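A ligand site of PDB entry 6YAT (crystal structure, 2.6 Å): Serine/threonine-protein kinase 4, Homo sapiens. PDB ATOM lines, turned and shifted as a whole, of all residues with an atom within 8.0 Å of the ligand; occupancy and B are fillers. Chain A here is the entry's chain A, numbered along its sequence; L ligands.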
ATOM      1  N   SER A  22      15.246  16.413  25.515  1.00  0.00           N
ATOM      2  CA  SER A  22      13.934  15.817  25.154  1.00  0.00           C
ATOM      3  C   SER A  22      13.459  14.872  26.265  1.00  0.00           C
ATOM      4  O   SER A  22      12.322  14.401  26.168  1.00  0.00           O
ATOM      5  CB  SER A  22      14.017  15.090  23.837  1.00  0.00           C
ATOM      6  OG  SER A  22      13.993  16.014  22.751  1.00  0.00           O
ATOM      7  N   LEU A  23      14.310  14.594  27.267  1.00  0.00           N
ATOM      8  CA  LEU A  23      14.096  13.507  28.261  1.00  0.00           C
ATOM      9  C   LEU A  23      13.486  14.069  29.549  1.00  0.00           C
ATOM     10  O   LEU A  23      12.903  13.285  30.314  1.00  0.00           O
ATOM     11  CB  LEU A  23      15.435  12.820  28.560  1.00  0.00           C
ATOM     12  CG  LEU A  23      15.976  11.907  27.452  1.00  0.00           C
ATOM     13  CD1 LEU A  23      17.265  11.234  27.893  1.00  0.00           C
ATOM     14  CD2 LEU A  23      14.943  10.871  27.042  1.00  0.00           C
ATOM     15  N   THR A  24      13.602  15.380  29.779  1.00  0.00           N
ATOM     16  CA  THR A  24      13.196  16.060  31.044  1.00  0.00           C
ATOM     17  C   THR A  24      12.076  17.087  30.769  1.00  0.00           C
ATOM     18  O   THR A  24      11.770  17.880  31.679  1.00  0.00           O
ATOM     19  CB  THR A  24      14.403  16.716  31.725  1.00  0.00           C
ATOM     20  OG1 THR A  24      14.899  17.734  30.853  1.00  0.00           O
ATOM     21  CG2 THR A  24      15.502  15.737  32.049  1.00  0.00           C
ATOM     22  N   LYS A  25      11.472  17.045  29.575  1.00  0.00           N
ATOM     23  CA  LYS A  25      10.303  17.897  29.202  1.00  0.00           C
ATOM     24  C   LYS A  25       9.210  17.698  30.246  1.00  0.00           C
ATOM     25  O   LYS A  25       8.847  16.543  30.493  1.00  0.00           O
ATOM     26  CB  LYS A  25       9.797  17.568  27.798  1.00  0.00           C
ATOM     27  CG  LYS A  25      10.237  18.542  26.708  1.00  0.00           C
ATOM     28  CD  LYS A  25       9.605  18.272  25.361  1.00  0.00           C
ATOM     29  CE  LYS A  25      10.445  18.773  24.195  1.00  0.00           C
ATOM     30  NZ  LYS A  25       9.939  18.286  22.893  1.00  0.00           N
ATOM     31  N   GLN A  26       8.713  18.790  30.847  1.00  0.00           N
ATOM     32  CA  GLN A  26       7.714  18.759  31.936  1.00  0.00           C
ATOM     33  C   GLN A  26       6.305  18.605  31.345  1.00  0.00           C
ATOM     34  O   GLN A  26       6.077  18.923  30.178  1.00  0.00           O
ATOM     35  CB  GLN A  26       7.835  20.021  32.798  1.00  0.00           C
ATOM     36  CG  GLN A  26       9.089  20.033  33.676  1.00  0.00           C
ATOM     37  CD  GLN A  26       8.768  20.239  35.129  1.00  0.00           C
ATOM     38  OE1 GLN A  26       7.930  21.071  35.497  1.00  0.00           O
ATOM     39  NE2 GLN A  26       9.422  19.472  35.985  1.00  0.00           N
ATOM     40  N   PRO A  27       5.334  18.071  32.117  1.00  0.00           N
ATOM     41  CA  PRO A  27       4.028  17.681  31.571  1.00  0.00           C
ATOM     42  C   PRO A  27       3.280  18.793  30.818  1.00  0.00           C
ATOM     43  O   PRO A  27       2.621  18.484  29.814  1.00  0.00           O
ATOM     44  CB  PRO A  27       3.244  17.262  32.824  1.00  0.00           C
ATOM     45  CG  PRO A  27       4.320  16.782  33.782  1.00  0.00           C
ATOM     46  CD  PRO A  27       5.478  17.726  33.538  1.00  0.00           C
ATOM     47  N   GLU A  29       4.586  20.998  29.122  1.00  0.00           N
ATOM     48  CA  GLU A  29       5.346  21.165  27.847  1.00  0.00           C
ATOM     49  C   GLU A  29       4.967  20.034  26.867  1.00  0.00           C
ATOM     50  O   GLU A  29       5.086  20.248  25.661  1.00  0.00           O
ATOM     51  CB  GLU A  29       6.859  21.146  28.097  1.00  0.00           C
ATOM     52  CG  GLU A  29       7.397  22.371  28.834  1.00  0.00           C
ATOM     53  CD  GLU A  29       8.933  22.419  28.946  1.00  0.00           C
ATOM     54  OE1 GLU A  29       9.536  21.457  29.519  1.00  0.00           O
ATOM     55  OE2 GLU A  29       9.545  23.428  28.475  1.00  0.00           O
ATOM     56  N   VAL A  30       4.592  18.859  27.374  1.00  0.00           N
ATOM     57  CA  VAL A  30       4.224  17.659  26.555  1.00  0.00           C
ATOM     58  C   VAL A  30       2.762  17.804  26.092  1.00  0.00           C
ATOM     59  O   VAL A  30       2.485  17.479  24.910  1.00  0.00           O
ATOM     60  CB  VAL A  30       4.425  16.350  27.345  1.00  0.00           C
ATOM     61  CG1 VAL A  30       4.007  15.146  26.519  1.00  0.00           C
ATOM     62  CG2 VAL A  30       5.862  16.197  27.823  1.00  0.00           C
ATOM     63  N   PHE A  31       1.861  18.208  27.000  1.00  0.00           N
ATOM     64  CA  PHE A  31       0.406  18.321  26.758  1.00  0.00           C
ATOM     65  C   PHE A  31       0.002  19.800  26.701  1.00  0.00           C
ATOM     66  O   PHE A  31       0.389  20.582  27.588  1.00  0.00           O
ATOM     67  CB  PHE A  31      -0.387  17.603  27.843  1.00  0.00           C
ATOM     68  CG  PHE A  31      -0.156  16.115  27.886  1.00  0.00           C
ATOM     69  CD1 PHE A  31      -0.677  15.285  26.905  1.00  0.00           C
ATOM     70  CD2 PHE A  31       0.606  15.551  28.897  1.00  0.00           C
ATOM     71  CE1 PHE A  31      -0.457  13.918  26.946  1.00  0.00           C
ATOM     72  CE2 PHE A  31       0.828  14.178  28.930  1.00  0.00           C
ATOM     73  CZ  PHE A  31       0.297  13.369  27.955  1.00  0.00           C
ATOM     74  N   HIS A  50      -1.644  15.901  23.090  1.00  0.00           N
ATOM     75  CA  HIS A  50      -0.211  15.526  22.964  1.00  0.00           C
ATOM     76  C   HIS A  50       0.424  16.362  21.847  1.00  0.00           C
ATOM     77  O   HIS A  50       0.254  15.987  20.678  1.00  0.00           O
ATOM     78  CB  HIS A  50      -0.080  14.023  22.727  1.00  0.00           C
ATOM     79  CG  HIS A  50       1.285  13.508  22.985  1.00  0.00           C
ATOM     80  ND1 HIS A  50       2.068  12.964  21.976  1.00  0.00           N
ATOM     81  CD2 HIS A  50       2.026  13.448  24.109  1.00  0.00           C
ATOM     82  CE1 HIS A  50       3.227  12.591  22.486  1.00  0.00           C
ATOM     83  NE2 HIS A  50       3.226  12.881  23.793  1.00  0.00           N
ATOM     84  N   LYS A  51       1.144  17.443  22.193  1.00  0.00           N
ATOM     85  CA  LYS A  51       1.665  18.466  21.240  1.00  0.00           C
ATOM     86  C   LYS A  51       2.391  17.765  20.087  1.00  0.00           C
ATOM     87  O   LYS A  51       2.286  18.251  18.944  1.00  0.00           O
ATOM     88  CB  LYS A  51       2.598  19.449  21.950  1.00  0.00           C
ATOM     89  CG  LYS A  51       1.882  20.564  22.703  1.00  0.00           C
ATOM     90  CD  LYS A  51       2.819  21.517  23.428  1.00  0.00           C
ATOM     91  CE  LYS A  51       2.072  22.653  24.114  1.00  0.00           C
ATOM     92  NZ  LYS A  51       2.806  23.141  25.312  1.00  0.00           N
ATOM     93  N   GLU A  52       3.052  16.638  20.372  1.00  0.00           N
ATOM     94  CA  GLU A  52       3.953  15.909  19.445  1.00  0.00           C
ATOM     95  C   GLU A  52       3.128  15.211  18.363  1.00  0.00           C
ATOM     96  O   GLU A  52       3.411  15.436  17.168  1.00  0.00           O
ATOM     97  CB  GLU A  52       4.803  14.922  20.242  1.00  0.00           C
ATOM     98  CG  GLU A  52       6.140  14.608  19.590  1.00  0.00           C
ATOM     99  CD  GLU A  52       6.932  13.517  20.306  1.00  0.00           C
ATOM    100  OE1 GLU A  52       6.571  13.180  21.449  1.00  0.00           O
ATOM    101  OE2 GLU A  52       7.883  13.008  19.708  1.00  0.00           O
ATOM    102  N   THR A  53       2.134  14.401  18.765  1.00  0.00           N
ATOM    103  CA  THR A  53       1.409  13.448  17.881  1.00  0.00           C
ATOM    104  C   THR A  53       0.045  14.039  17.458  1.00  0.00           C
ATOM    105  O   THR A  53      -0.596  13.457  16.568  1.00  0.00           O
ATOM    106  CB  THR A  53       1.206  12.092  18.574  1.00  0.00           C
ATOM    107  OG1 THR A  53       0.460  12.308  19.765  1.00  0.00           O
ATOM    108  CG2 THR A  53       2.513  11.411  18.916  1.00  0.00           C
ATOM    109  N   SER A  92       0.895   7.897  33.098  1.00  0.00           N
ATOM    110  CA  SER A  92       0.892   8.854  34.237  1.00  0.00           C
ATOM    111  C   SER A  92       2.100   9.804  34.148  1.00  0.00           C
ATOM    112  O   SER A  92       3.136   9.403  33.648  1.00  0.00           O
ATOM    113  CB  SER A  92       0.874   8.113  35.559  1.00  0.00           C
ATOM    114  OG  SER A  92      -0.274   7.266  35.649  1.00  0.00           O
ATOM    115  N   TYR A  93       1.941  11.034  34.626  1.00  0.00           N
ATOM    116  CA  TYR A  93       2.999  12.071  34.726  1.00  0.00           C
ATOM    117  C   TYR A  93       2.880  12.748  36.082  1.00  0.00           C
ATOM    118  O   TYR A  93       1.777  12.867  36.590  1.00  0.00           O
ATOM    119  CB  TYR A  93       2.880  13.082  33.596  1.00  0.00           C
ATOM    120  CG  TYR A  93       2.936  12.512  32.200  1.00  0.00           C
ATOM    121  CD1 TYR A  93       1.824  11.883  31.636  1.00  0.00           C
ATOM    122  CD2 TYR A  93       4.077  12.639  31.408  1.00  0.00           C
ATOM    123  CE1 TYR A  93       1.861  11.362  30.355  1.00  0.00           C
ATOM    124  CE2 TYR A  93       4.110  12.147  30.113  1.00  0.00           C
ATOM    125  CZ  TYR A  93       3.007  11.494  29.587  1.00  0.00           C
ATOM    126  OH  TYR A  93       3.022  10.988  28.316  1.00  0.00           O
HETATM  127  O1  LIG L   1       5.736  11.421  27.397  1.00  0.00           O
HETATM  128  O2  LIG L   1       5.254  10.760  25.111  1.00  0.00           O
HETATM  129  O3  LIG L   1       8.330  11.114  28.051  1.00  0.00           O
HETATM  130  O4  LIG L   1       6.117  13.022  25.591  1.00  0.00           O
HETATM  131  C1  LIG L   1      13.772   6.915  28.303  1.00  0.00           C
HETATM  132  C2  LIG L   1      12.642   6.528  29.237  1.00  0.00           C
HETATM  133  C3  LIG L   1      13.240   7.246  26.924  1.00  0.00           C
HETATM  134  C4  LIG L   1      11.586   7.623  29.309  1.00  0.00           C
HETATM  135  C5  LIG L   1      12.177   8.350  26.987  1.00  0.00           C
HETATM  136  C6  LIG L   1       9.471   9.463  26.740  1.00  0.00           C
HETATM  137  C7  LIG L   1       7.743  11.022  25.747  1.00  0.00           C
HETATM  138  N1  LIG L   1      10.045   9.031  28.014  1.00  0.00           N
HETATM  139  C8  LIG L   1       8.179  10.220  26.959  1.00  0.00           C
HETATM  140  C9  LIG L   1      11.047   7.962  27.921  1.00  0.00           C
HETATM  141  S1  LIG L   1       6.080  11.615  25.901  1.00  0.00           S
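CD2 of Leu 23 touches C5 of the ligand (3.7 Å).
Val 30 touches the ligand.
O2 of the ligand lies within hydrogen-bond range of NE2 of His 50, at 3.2 Å.
The side-chain hydroxyl (OH) of Tyr 93 sits at hydrogen-bond distance from an oxygen (O1) of the ligand, at 2.9 Å.
ND1 of His 50 lies within hydrogen-bond range of OG1 of Thr 53, 2.8 Å away.
O of Val 30 is in hydrogen-bond range of N of Lys 51 (3.0 Å).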
